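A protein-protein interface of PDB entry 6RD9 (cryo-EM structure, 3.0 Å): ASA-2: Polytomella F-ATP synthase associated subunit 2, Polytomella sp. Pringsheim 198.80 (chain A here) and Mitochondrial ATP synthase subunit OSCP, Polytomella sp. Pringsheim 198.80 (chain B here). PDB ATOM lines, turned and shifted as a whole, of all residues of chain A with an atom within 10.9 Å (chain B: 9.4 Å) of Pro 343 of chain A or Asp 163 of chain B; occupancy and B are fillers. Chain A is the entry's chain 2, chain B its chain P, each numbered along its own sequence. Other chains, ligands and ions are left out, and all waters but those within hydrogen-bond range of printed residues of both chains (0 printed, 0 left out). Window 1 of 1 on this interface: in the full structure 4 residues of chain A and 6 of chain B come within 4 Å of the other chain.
Among the printed residues, pairs that only touch across the chains: Glu 344 of chain A with Leu 165 of chain B, Pro 343 of chain A with Glu 169 of chain B, Tyr 341 of chain A with Asp 163 of chain B, Tyr 341 of chain A with Leu 165 of chain B, Pro 343 of chain A with Glu 166 of chain B, Pro 343 of chain A with Asp 163 of chain B and Pro 343 of chain A with Leu 165 of chain B.
Hydrophobic or aromatic side chains of chain A that line the printed part of chain B: Tyr 341 and Pro 343. Of the 15 printed residues of chain B, 6 touch a printed residue of chain A. Hydrophobic or aromatic side chains of chain B that line the printed part of chain A: Leu 165. Among the printed residues, Asp or Glu carboxylates within 4 Å of a Lys or Arg side-chain nitrogen of the other chain: Arg 342 of chain A with Glu 160 of chain B, Arg 342 of chain A with Asp 163 of chain B and Arg 342 of chain A with Glu 166 of chain B.
OE2 of Glu 160 of chain B is in salt-bridge range of NH2 of Arg 342 of chain A. The guanidinium group of Arg 342 of chain A is in hydrogen-bond range of the backbone carbonyl oxygen of Pro 161 of chain B (3.0 Å). OD1 of Asp 163 of chain B lies within salt-bridge range of NH1 of Arg 342 of chain A. NH1 of Arg 342 of chain A lies within salt-bridge range of OE1 of Glu 166 of chain B, at 2.4 Å.
Of chain B, only Asp 163 (3.9 Å), Leu 165 (3.96 Å), Glu 166 (3.9 Å) and Glu 169 (3.3 Å) come within 4 Å of Pro 343 of chain A. Of chain A, only Tyr 341 (3.6 Å), Arg 342 (2.9 Å) and Pro 343 (3.9 Å) come within 4 Å of Asp 163 of chain B. Of chain B, only Glu 160 (3.2 Å), Pro 161 (3.0 Å), Asp 163 (2.9 Å) and Glu 166 (2.4 Å) come within 4 Å of Arg 342 of chain A. No residue of chain A comes within 4 Å of Leu 162 of chain B. Printed residues of chain A within 4 Å of Leu 165 of chain B: Tyr 341, Pro 343 and Glu 344. Glu 166 of chain B touches just these residues of chain A: Arg 342 (2.4 Å) and Pro 343 (3.9 Å). Of the printed residues of chain A, Pro 161 of chain B touches Arg 342 (3.0 Å). Printed residues of chain B within 4 Å of Tyr 341 of chain A: Asp 163 and Leu 165. Of the printed residues of chain A, Glu 160 of chain B touches Arg 342 (3.2 Å). Printed residues of chain B within 4 Å of Glu 344 of chain A: Leu 165 (3.3 Å). Ala 346 of chain A touches none of the printed residues of chain B. The nearest residue of chain B that does not touch Pro 343 of chain A is Arg 167 of chain B (6.9 Å). The nearest residue of chain A that does not touch Asp 163 of chain B is Gln 340 of chain A (5.2 Å).
The backbone carbonyl oxygen (O) of Glu 160 of chain B lies within hydrogen-bond range of the side-chain hydroxyl (OG1) of Thr 158 of chain B (3.3 Å). The side-chain carboxylate of Glu 166 of chain B sits at hydrogen-bond distance from the backbone NH of Asp 163 of chain B, at 3.4 Å. The guanidinium group (NH1) of Arg 167 of chain B is in hydrogen-bond range of the backbone carbonyl oxygen (O) of Asp 163 of chain B (2.9 Å). The side-chain carboxylate (OE1) of Glu 344 of chain A sits at hydrogen-bond distance from the backbone NH (N) of Gln 340 of chain A (2.7 Å). The backbone NH (N) of Tyr 341 of chain A lies within hydrogen-bond range of the side-chain carboxylate (OE1) of Glu 344 of chain A.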
ATOM      1  N   ALA A 331      -9.486  36.276  -2.746  1.00  0.00           N
ATOM      2  CA  ALA A 331      -8.979  35.359  -1.734  1.00  0.00           C
ATOM      3  C   ALA A 331      -8.199  36.099  -0.661  1.00  0.00           C
ATOM      4  O   ALA A 331      -8.283  35.753   0.521  1.00  0.00           O
ATOM      5  CB  ALA A 331      -8.103  34.292  -2.380  1.00  0.00           C
ATOM      6  N   ALA A 334     -10.577  37.571   1.555  1.00  0.00           N
ATOM      7  CA  ALA A 334     -11.089  36.620   2.534  1.00  0.00           C
ATOM      8  C   ALA A 334     -10.133  36.472   3.711  1.00  0.00           C
ATOM      9  O   ALA A 334     -10.568  36.417   4.864  1.00  0.00           O
ATOM     10  CB  ALA A 334     -11.346  35.270   1.873  1.00  0.00           C
ATOM     11  N   VAL A 335      -8.828  36.415   3.439  1.00  0.00           N
ATOM     12  CA  VAL A 335      -7.832  36.277   4.492  1.00  0.00           C
ATOM     13  C   VAL A 335      -7.704  37.555   5.312  1.00  0.00           C
ATOM     14  O   VAL A 335      -7.500  37.490   6.529  1.00  0.00           O
ATOM     15  CB  VAL A 335      -6.497  35.858   3.843  1.00  0.00           C
ATOM     16  CG1 VAL A 335      -5.353  35.842   4.821  1.00  0.00           C
ATOM     17  CG2 VAL A 335      -6.644  34.499   3.243  1.00  0.00           C
ATOM     18  N   GLY A 338     -10.494  37.651   7.800  1.00  0.00           N
ATOM     19  CA  GLY A 338     -10.348  36.595   8.775  1.00  0.00           C
ATOM     20  C   GLY A 338     -10.831  35.278   8.230  1.00  0.00           C
ATOM     21  O   GLY A 338     -12.006  34.925   8.363  1.00  0.00           O
ATOM     22  N   ALA A 339      -9.903  34.539   7.631  1.00  0.00           N
ATOM     23  CA  ALA A 339     -10.161  33.206   7.101  1.00  0.00           C
ATOM     24  C   ALA A 339      -8.798  32.571   6.879  1.00  0.00           C
ATOM     25  O   ALA A 339      -8.100  32.948   5.936  1.00  0.00           O
ATOM     26  CB  ALA A 339     -10.953  33.268   5.804  1.00  0.00           C
ATOM     27  N   GLN A 340      -8.415  31.624   7.724  1.00  0.00           N
ATOM     28  CA  GLN A 340      -7.089  31.046   7.596  1.00  0.00           C
ATOM     29  C   GLN A 340      -7.089  29.700   6.897  1.00  0.00           C
ATOM     30  O   GLN A 340      -6.015  29.204   6.548  1.00  0.00           O
ATOM     31  CB  GLN A 340      -6.429  30.907   8.974  1.00  0.00           C
ATOM     32  CG  GLN A 340      -7.060  29.866   9.872  1.00  0.00           C
ATOM     33  CD  GLN A 340      -8.207  30.410  10.695  1.00  0.00           C
ATOM     34  OE1 GLN A 340      -8.717  31.498  10.437  1.00  0.00           O
ATOM     35  NE2 GLN A 340      -8.627  29.644  11.691  1.00  0.00           N
ATOM     36  N   TYR A 341      -8.252  29.112   6.659  1.00  0.00           N
ATOM     37  CA  TYR A 341      -8.330  27.795   6.057  1.00  0.00           C
ATOM     38  C   TYR A 341      -9.087  27.852   4.742  1.00  0.00           C
ATOM     39  O   TYR A 341      -9.891  28.756   4.503  1.00  0.00           O
ATOM     40  CB  TYR A 341      -8.981  26.799   7.010  1.00  0.00           C
ATOM     41  CG  TYR A 341      -8.173  26.625   8.268  1.00  0.00           C
ATOM     42  CD1 TYR A 341      -6.798  26.468   8.202  1.00  0.00           C
ATOM     43  CD2 TYR A 341      -8.779  26.634   9.512  1.00  0.00           C
ATOM     44  CE1 TYR A 341      -6.047  26.317   9.339  1.00  0.00           C
ATOM     45  CE2 TYR A 341      -8.037  26.486  10.655  1.00  0.00           C
ATOM     46  CZ  TYR A 341      -6.671  26.328  10.565  1.00  0.00           C
ATOM     47  OH  TYR A 341      -5.921  26.179  11.709  1.00  0.00           O
ATOM     48  N   ARG A 342      -8.804  26.871   3.890  1.00  0.00           N
ATOM     49  CA  ARG A 342      -9.350  26.872   2.539  1.00  0.00           C
ATOM     50  C   ARG A 342     -10.863  26.678   2.430  1.00  0.00           C
ATOM     51  O   ARG A 342     -11.439  27.270   1.506  1.00  0.00           O
ATOM     52  CB  ARG A 342      -8.602  25.830   1.699  1.00  0.00           C
ATOM     53  CG  ARG A 342      -7.131  26.150   1.562  1.00  0.00           C
ATOM     54  CD  ARG A 342      -6.497  25.316   0.482  1.00  0.00           C
ATOM     55  NE  ARG A 342      -6.374  23.922   0.879  1.00  0.00           N
ATOM     56  CZ  ARG A 342      -5.216  23.326   1.118  1.00  0.00           C
ATOM     57  NH1 ARG A 342      -5.184  22.052   1.476  1.00  0.00           N
ATOM     58  NH2 ARG A 342      -4.090  24.010   0.989  1.00  0.00           N
ATOM     59  N   PRO A 343     -11.564  25.899   3.273  1.00  0.00           N
ATOM     60  CA  PRO A 343     -13.035  25.960   3.226  1.00  0.00           C
ATOM     61  C   PRO A 343     -13.614  27.291   3.660  1.00  0.00           C
ATOM     62  O   PRO A 343     -14.772  27.577   3.336  1.00  0.00           O
ATOM     63  CB  PRO A 343     -13.466  24.841   4.177  1.00  0.00           C
ATOM     64  CG  PRO A 343     -12.392  23.889   4.105  1.00  0.00           C
ATOM     65  CD  PRO A 343     -11.143  24.697   4.021  1.00  0.00           C
ATOM     66  N   GLU A 344     -12.863  28.102   4.399  1.00  0.00           N
ATOM     67  CA  GLU A 344     -13.339  29.435   4.728  1.00  0.00           C
ATOM     68  C   GLU A 344     -13.207  30.378   3.540  1.00  0.00           C
ATOM     69  O   GLU A 344     -14.157  31.097   3.209  1.00  0.00           O
ATOM     70  CB  GLU A 344     -12.570  29.980   5.924  1.00  0.00           C
ATOM     71  CG  GLU A 344     -12.759  29.230   7.214  1.00  0.00           C
ATOM     72  CD  GLU A 344     -11.553  29.357   8.116  1.00  0.00           C
ATOM     73  OE1 GLU A 344     -10.557  29.971   7.687  1.00  0.00           O
ATOM     74  OE2 GLU A 344     -11.608  28.874   9.261  1.00  0.00           O
ATOM     75  N   VAL A 345     -12.043  30.385   2.877  1.00  0.00           N
ATOM     76  CA  VAL A 345     -11.838  31.317   1.773  1.00  0.00           C
ATOM     77  C   VAL A 345     -12.643  30.889   0.555  1.00  0.00           C
ATOM     78  O   VAL A 345     -12.999  31.717  -0.282  1.00  0.00           O
ATOM     79  CB  VAL A 345     -10.342  31.481   1.431  1.00  0.00           C
ATOM     80  CG1 VAL A 345      -9.566  31.927   2.626  1.00  0.00           C
ATOM     81  CG2 VAL A 345      -9.742  30.224   0.872  1.00  0.00           C
ATOM     82  N   ALA A 346     -12.963  29.602   0.438  1.00  0.00           N
ATOM     83  CA  ALA A 346     -13.765  29.177  -0.698  1.00  0.00           C
ATOM     84  C   ALA A 346     -15.215  29.597  -0.540  1.00  0.00           C
ATOM     85  O   ALA A 346     -15.891  29.868  -1.536  1.00  0.00           O
ATOM     86  CB  ALA A 346     -13.672  27.669  -0.883  1.00  0.00           C
ATOM     87  N   SER A 347     -15.707  29.666   0.687  1.00  0.00           N
ATOM     88  CA  SER A 347     -17.078  30.077   0.926  1.00  0.00           C
ATOM     89  C   SER A 347     -17.196  31.555   1.253  1.00  0.00           C
ATOM     90  O   SER A 347     -18.316  32.057   1.379  1.00  0.00           O
ATOM     91  CB  SER A 347     -17.690  29.245   2.054  1.00  0.00           C
ATOM     92  OG  SER A 347     -18.823  29.891   2.604  1.00  0.00           O
ATOM     93  N   ALA A 348     -16.075  32.261   1.401  1.00  0.00           N
ATOM     94  CA  ALA A 348     -16.136  33.706   1.568  1.00  0.00           C
ATOM     95  C   ALA A 348     -16.193  34.426   0.232  1.00  0.00           C
ATOM     96  O   ALA A 348     -17.000  35.345   0.064  1.00  0.00           O
ATOM     97  CB  ALA A 348     -14.934  34.205   2.370  1.00  0.00           C
ATOM     98  N   VAL A 349     -15.382  33.993  -0.740  1.00  0.00           N
ATOM     99  CA  VAL A 349     -15.357  34.643  -2.042  1.00  0.00           C
ATOM    100  C   VAL A 349     -16.576  34.296  -2.874  1.00  0.00           C
ATOM    101  O   VAL A 349     -16.791  34.901  -3.922  1.00  0.00           O
ATOM    102  CB  VAL A 349     -14.074  34.294  -2.813  1.00  0.00           C
ATOM    103  CG1 VAL A 349     -12.877  34.480  -1.949  1.00  0.00           C
ATOM    104  CG2 VAL A 349     -14.129  32.895  -3.337  1.00  0.00           C
ATOM    105  N   ALA A 350     -17.380  33.337  -2.452  1.00  0.00           N
ATOM    106  CA  ALA A 350     -18.688  33.148  -3.050  1.00  0.00           C
ATOM    107  C   ALA A 350     -19.743  34.016  -2.391  1.00  0.00           C
ATOM    108  O   ALA A 350     -20.897  34.004  -2.824  1.00  0.00           O
ATOM    109  CB  ALA A 350     -19.103  31.680  -2.971  1.00  0.00           C
ATOM    110  N   SER A 351     -19.383  34.738  -1.341  1.00  0.00           N
ATOM    111  CA  SER A 351     -20.272  35.706  -0.725  1.00  0.00           C
ATOM    112  C   SER A 351     -19.896  37.132  -1.072  1.00  0.00           C
ATOM    113  O   SER A 351     -20.636  38.057  -0.729  1.00  0.00           O
ATOM    114  CB  SER A 351     -20.262  35.542   0.794  1.00  0.00           C
ATOM    115  OG  SER A 351     -18.943  35.671   1.292  1.00  0.00           O
ATOM    116  N   GLN A 423       0.560  35.146   0.532  1.00  0.00           N
ATOM    117  CA  GLN A 423      -0.835  35.523   0.708  1.00  0.00           C
ATOM    118  C   GLN A 423      -1.048  36.404   1.931  1.00  0.00           C
ATOM    119  O   GLN A 423      -2.044  37.133   1.995  1.00  0.00           O
ATOM    120  CB  GLN A 423      -1.706  34.271   0.805  1.00  0.00           C
ATOM    121  CG  GLN A 423      -3.176  34.504   0.526  1.00  0.00           C
ATOM    122  CD  GLN A 423      -3.969  33.226   0.500  1.00  0.00           C
ATOM    123  OE1 GLN A 423      -5.194  33.242   0.549  1.00  0.00           O
ATOM    124  NE2 GLN A 423      -3.274  32.105   0.414  1.00  0.00           N
ATOM    125  N   THR B 158      -5.663  13.203  -1.488  1.00  0.00           N
ATOM    126  CA  THR B 158      -6.027  14.571  -1.821  1.00  0.00           C
ATOM    127  C   THR B 158      -4.989  15.161  -2.771  1.00  0.00           C
ATOM    128  O   THR B 158      -4.085  14.477  -3.240  1.00  0.00           O
ATOM    129  CB  THR B 158      -6.161  15.411  -0.551  1.00  0.00           C
ATOM    130  OG1 THR B 158      -4.978  15.258   0.239  1.00  0.00           O
ATOM    131  CG2 THR B 158      -7.357  14.976   0.253  1.00  0.00           C
ATOM    132  N   GLU B 160      -3.185  18.438  -2.316  1.00  0.00           N
ATOM    133  CA  GLU B 160      -2.123  18.933  -1.458  1.00  0.00           C
ATOM    134  C   GLU B 160      -2.499  18.584  -0.026  1.00  0.00           C
ATOM    135  O   GLU B 160      -3.661  18.255   0.238  1.00  0.00           O
ATOM    136  CB  GLU B 160      -1.935  20.450  -1.640  1.00  0.00           C
ATOM    137  CG  GLU B 160      -3.066  21.308  -1.119  1.00  0.00           C
ATOM    138  CD  GLU B 160      -4.111  21.606  -2.171  1.00  0.00           C
ATOM    139  OE1 GLU B 160      -4.121  20.930  -3.216  1.00  0.00           O
ATOM    140  OE2 GLU B 160      -4.921  22.529  -1.958  1.00  0.00           O
ATOM    141  N   PRO B 161      -1.533  18.582   0.913  1.00  0.00           N
ATOM    142  CA  PRO B 161      -1.854  18.231   2.305  1.00  0.00           C
ATOM    143  C   PRO B 161      -2.869  19.161   2.948  1.00  0.00           C
ATOM    144  O   PRO B 161      -2.983  20.338   2.605  1.00  0.00           O
ATOM    145  CB  PRO B 161      -0.503  18.320   3.010  1.00  0.00           C
ATOM    146  CG  PRO B 161       0.452  17.945   1.981  1.00  0.00           C
ATOM    147  CD  PRO B 161      -0.075  18.529   0.695  1.00  0.00           C
ATOM    148  N   LEU B 162      -3.622  18.594   3.881  1.00  0.00           N
ATOM    149  CA  LEU B 162      -4.855  19.182   4.360  1.00  0.00           C
ATOM    150  C   LEU B 162      -4.601  20.244   5.421  1.00  0.00           C
ATOM    151  O   LEU B 162      -3.527  20.336   6.018  1.00  0.00           O
ATOM    152  CB  LEU B 162      -5.764  18.108   4.942  1.00  0.00           C
ATOM    153  CG  LEU B 162      -6.204  16.963   4.045  1.00  0.00           C
ATOM    154  CD1 LEU B 162      -5.381  15.733   4.336  1.00  0.00           C
ATOM    155  CD2 LEU B 162      -7.664  16.703   4.293  1.00  0.00           C
ATOM    156  N   ASP B 163      -5.636  21.044   5.658  1.00  0.00           N
ATOM    157  CA  ASP B 163      -5.717  21.909   6.817  1.00  0.00           C
ATOM    158  C   ASP B 163      -6.172  21.089   8.016  1.00  0.00           C
ATOM    159  O   ASP B 163      -6.381  19.877   7.928  1.00  0.00           O
ATOM    160  CB  ASP B 163      -6.692  23.052   6.556  1.00  0.00           C
ATOM    161  CG  ASP B 163      -6.425  23.762   5.244  1.00  0.00           C
ATOM    162  OD1 ASP B 163      -5.335  23.566   4.672  1.00  0.00           O
ATOM    163  OD2 ASP B 163      -7.311  24.505   4.778  1.00  0.00           O
ATOM    164  N   LYS B 164      -6.345  21.741   9.153  1.00  0.00           N
ATOM    165  CA  LYS B 164      -7.061  21.071  10.221  1.00  0.00           C
ATOM    166  C   LYS B 164      -8.564  21.221  10.055  1.00  0.00           C
ATOM    167  O   LYS B 164      -9.317  20.503  10.713  1.00  0.00           O
ATOM    168  CB  LYS B 164      -6.599  21.586  11.594  1.00  0.00           C
ATOM    169  CG  LYS B 164      -5.166  21.261  12.011  1.00  0.00           C
ATOM    170  CD  LYS B 164      -4.823  21.849  13.383  1.00  0.00           C
ATOM    171  CE  LYS B 164      -3.417  21.505  13.797  1.00  0.00           C
ATOM    172  NZ  LYS B 164      -3.089  22.098  15.114  1.00  0.00           N
ATOM    173  N   LEU B 165      -9.013  22.151   9.213  1.00  0.00           N
ATOM    174  CA  LEU B 165     -10.434  22.243   8.906  1.00  0.00           C
ATOM    175  C   LEU B 165     -10.769  21.394   7.693  1.00  0.00           C
ATOM    176  O   LEU B 165     -11.877  20.858   7.597  1.00  0.00           O
ATOM    177  CB  LEU B 165     -10.839  23.699   8.678  1.00  0.00           C
ATOM    178  CG  LEU B 165     -12.271  24.181   8.965  1.00  0.00           C
ATOM    179  CD1 LEU B 165     -12.266  25.679   8.977  1.00  0.00           C
ATOM    180  CD2 LEU B 165     -13.337  23.722   7.977  1.00  0.00           C
ATOM    181  N   GLU B 166      -9.815  21.239   6.772  1.00  0.00           N
ATOM    182  CA  GLU B 166     -10.001  20.303   5.669  1.00  0.00           C
ATOM    183  C   GLU B 166     -10.057  18.864   6.162  1.00  0.00           C
ATOM    184  O   GLU B 166     -10.649  18.006   5.503  1.00  0.00           O
ATOM    185  CB  GLU B 166      -8.884  20.467   4.640  1.00  0.00           C
ATOM    186  CG  GLU B 166      -9.261  21.370   3.479  1.00  0.00           C
ATOM    187  CD  GLU B 166      -8.266  21.304   2.336  1.00  0.00           C
ATOM    188  OE1 GLU B 166      -7.087  20.982   2.583  1.00  0.00           O
ATOM    189  OE2 GLU B 166      -8.669  21.569   1.184  1.00  0.00           O
ATOM    190  N   ARG B 167      -9.443  18.585   7.310  1.00  0.00           N
ATOM    191  CA  ARG B 167      -9.602  17.287   7.946  1.00  0.00           C
ATOM    192  C   ARG B 167     -10.999  17.118   8.527  1.00  0.00           C
ATOM    193  O   ARG B 167     -11.588  16.039   8.427  1.00  0.00           O
ATOM    194  CB  ARG B 167      -8.551  17.122   9.035  1.00  0.00           C
ATOM    195  CG  ARG B 167      -8.350  15.714   9.516  1.00  0.00           C
ATOM    196  CD  ARG B 167      -7.000  15.570  10.193  1.00  0.00           C
ATOM    197  NE  ARG B 167      -5.910  15.455   9.230  1.00  0.00           N
ATOM    198  CZ  ARG B 167      -5.097  16.449   8.890  1.00  0.00           C
ATOM    199  NH1 ARG B 167      -5.250  17.647   9.427  1.00  0.00           N
ATOM    200  NH2 ARG B 167      -4.133  16.247   8.006  1.00  0.00           N
ATOM    201  N   VAL B 168     -11.548  18.166   9.137  1.00  0.00           N
ATOM    202  CA  VAL B 168     -12.794  17.997   9.878  1.00  0.00           C
ATOM    203  C   VAL B 168     -13.999  17.985   8.943  1.00  0.00           C
ATOM    204  O   VAL B 168     -14.966  17.251   9.180  1.00  0.00           O
ATOM    205  CB  VAL B 168     -12.886  19.091  10.960  1.00  0.00           C
ATOM    206  CG1 VAL B 168     -14.230  19.099  11.660  1.00  0.00           C
ATOM    207  CG2 VAL B 168     -11.805  18.866  11.995  1.00  0.00           C
ATOM    208  N   GLU B 169     -13.945  18.738   7.844  1.00  0.00           N
ATOM    209  CA  GLU B 169     -15.048  18.744   6.886  1.00  0.00           C
ATOM    210  C   GLU B 169     -15.106  17.434   6.112  1.00  0.00           C
ATOM    211  O   GLU B 169     -16.149  17.072   5.557  1.00  0.00           O
ATOM    212  CB  GLU B 169     -14.913  19.924   5.924  1.00  0.00           C
ATOM    213  CG  GLU B 169     -13.663  19.876   5.064  1.00  0.00           C
ATOM    214  CD  GLU B 169     -13.817  20.588   3.736  1.00  0.00           C
ATOM    215  OE1 GLU B 169     -14.952  20.968   3.378  1.00  0.00           O
ATOM    216  OE2 GLU B 169     -12.791  20.762   3.045  1.00  0.00           O
ATOM    217  N   LEU B 170     -13.987  16.716   6.061  1.00  0.00           N
ATOM    218  CA  LEU B 170     -13.879  15.517   5.244  1.00  0.00           C
ATOM    219  C   LEU B 170     -14.453  14.292   5.937  1.00  0.00           C
ATOM    220  O   LEU B 170     -15.045  13.441   5.270  1.00  0.00           O
ATOM    221  CB  LEU B 170     -12.413  15.292   4.889  1.00  0.00           C
ATOM    222  CG  LEU B 170     -11.891  14.059   4.170  1.00  0.00           C
ATOM    223  CD1 LEU B 170     -12.716  13.685   2.971  1.00  0.00           C
ATOM    224  CD2 LEU B 170     -10.500  14.394   3.749  1.00  0.00           C
ATOM    225  N   LYS B 173     -17.987  14.123   5.423  1.00  0.00           N
ATOM    226  CA  LYS B 173     -18.316  13.468   4.163  1.00  0.00           C
ATOM    227  C   LYS B 173     -18.187  11.958   4.288  1.00  0.00           C
ATOM    228  O   LYS B 173     -19.031  11.209   3.784  1.00  0.00           O
ATOM    229  CB  LYS B 173     -17.390  13.968   3.056  1.00  0.00           C
ATOM    230  CG  LYS B 173     -17.484  15.436   2.735  1.00  0.00           C
ATOM    231  CD  LYS B 173     -18.730  15.753   1.943  1.00  0.00           C
ATOM    232  CE  LYS B 173     -18.774  17.224   1.591  1.00  0.00           C
ATOM    233  NZ  LYS B 173     -17.651  17.582   0.685  1.00  0.00           N
ATOM    234  N   MET B 186      -8.129   7.105   9.383  1.00  0.00           N
ATOM    235  CA  MET B 186      -7.990   7.725   8.062  1.00  0.00           C
ATOM    236  C   MET B 186      -6.560   7.366   7.667  1.00  0.00           C
ATOM    237  O   MET B 186      -5.798   6.895   8.514  1.00  0.00           O
ATOM    238  CB  MET B 186      -8.254   9.238   8.014  1.00  0.00           C
ATOM    239  CG  MET B 186      -8.514   9.793   6.611  1.00  0.00           C
ATOM    240  SD  MET B 186      -8.996  11.522   6.542  1.00  0.00           S
ATOM    241  CE  MET B 186     -10.713  11.384   7.016  1.00  0.00           C
ATOM    242  N   GLU B 188      -3.728   9.562   5.102  1.00  0.00           N
ATOM    243  CA  GLU B 188      -3.705  10.733   4.238  1.00  0.00           C
ATOM    244  C   GLU B 188      -2.530  10.649   3.274  1.00  0.00           C
ATOM    245  O   GLU B 188      -1.373  10.581   3.698  1.00  0.00           O
ATOM    246  CB  GLU B 188      -3.649  12.002   5.084  1.00  0.00           C
ATOM    247  CG  GLU B 188      -4.909  12.185   5.907  1.00  0.00           C
ATOM    248  CD  GLU B 188      -4.818  13.326   6.898  1.00  0.00           C
ATOM    249  OE1 GLU B 188      -3.715  13.881   7.078  1.00  0.00           O
ATOM    250  OE2 GLU B 188      -5.858  13.675   7.497  1.00  0.00           O
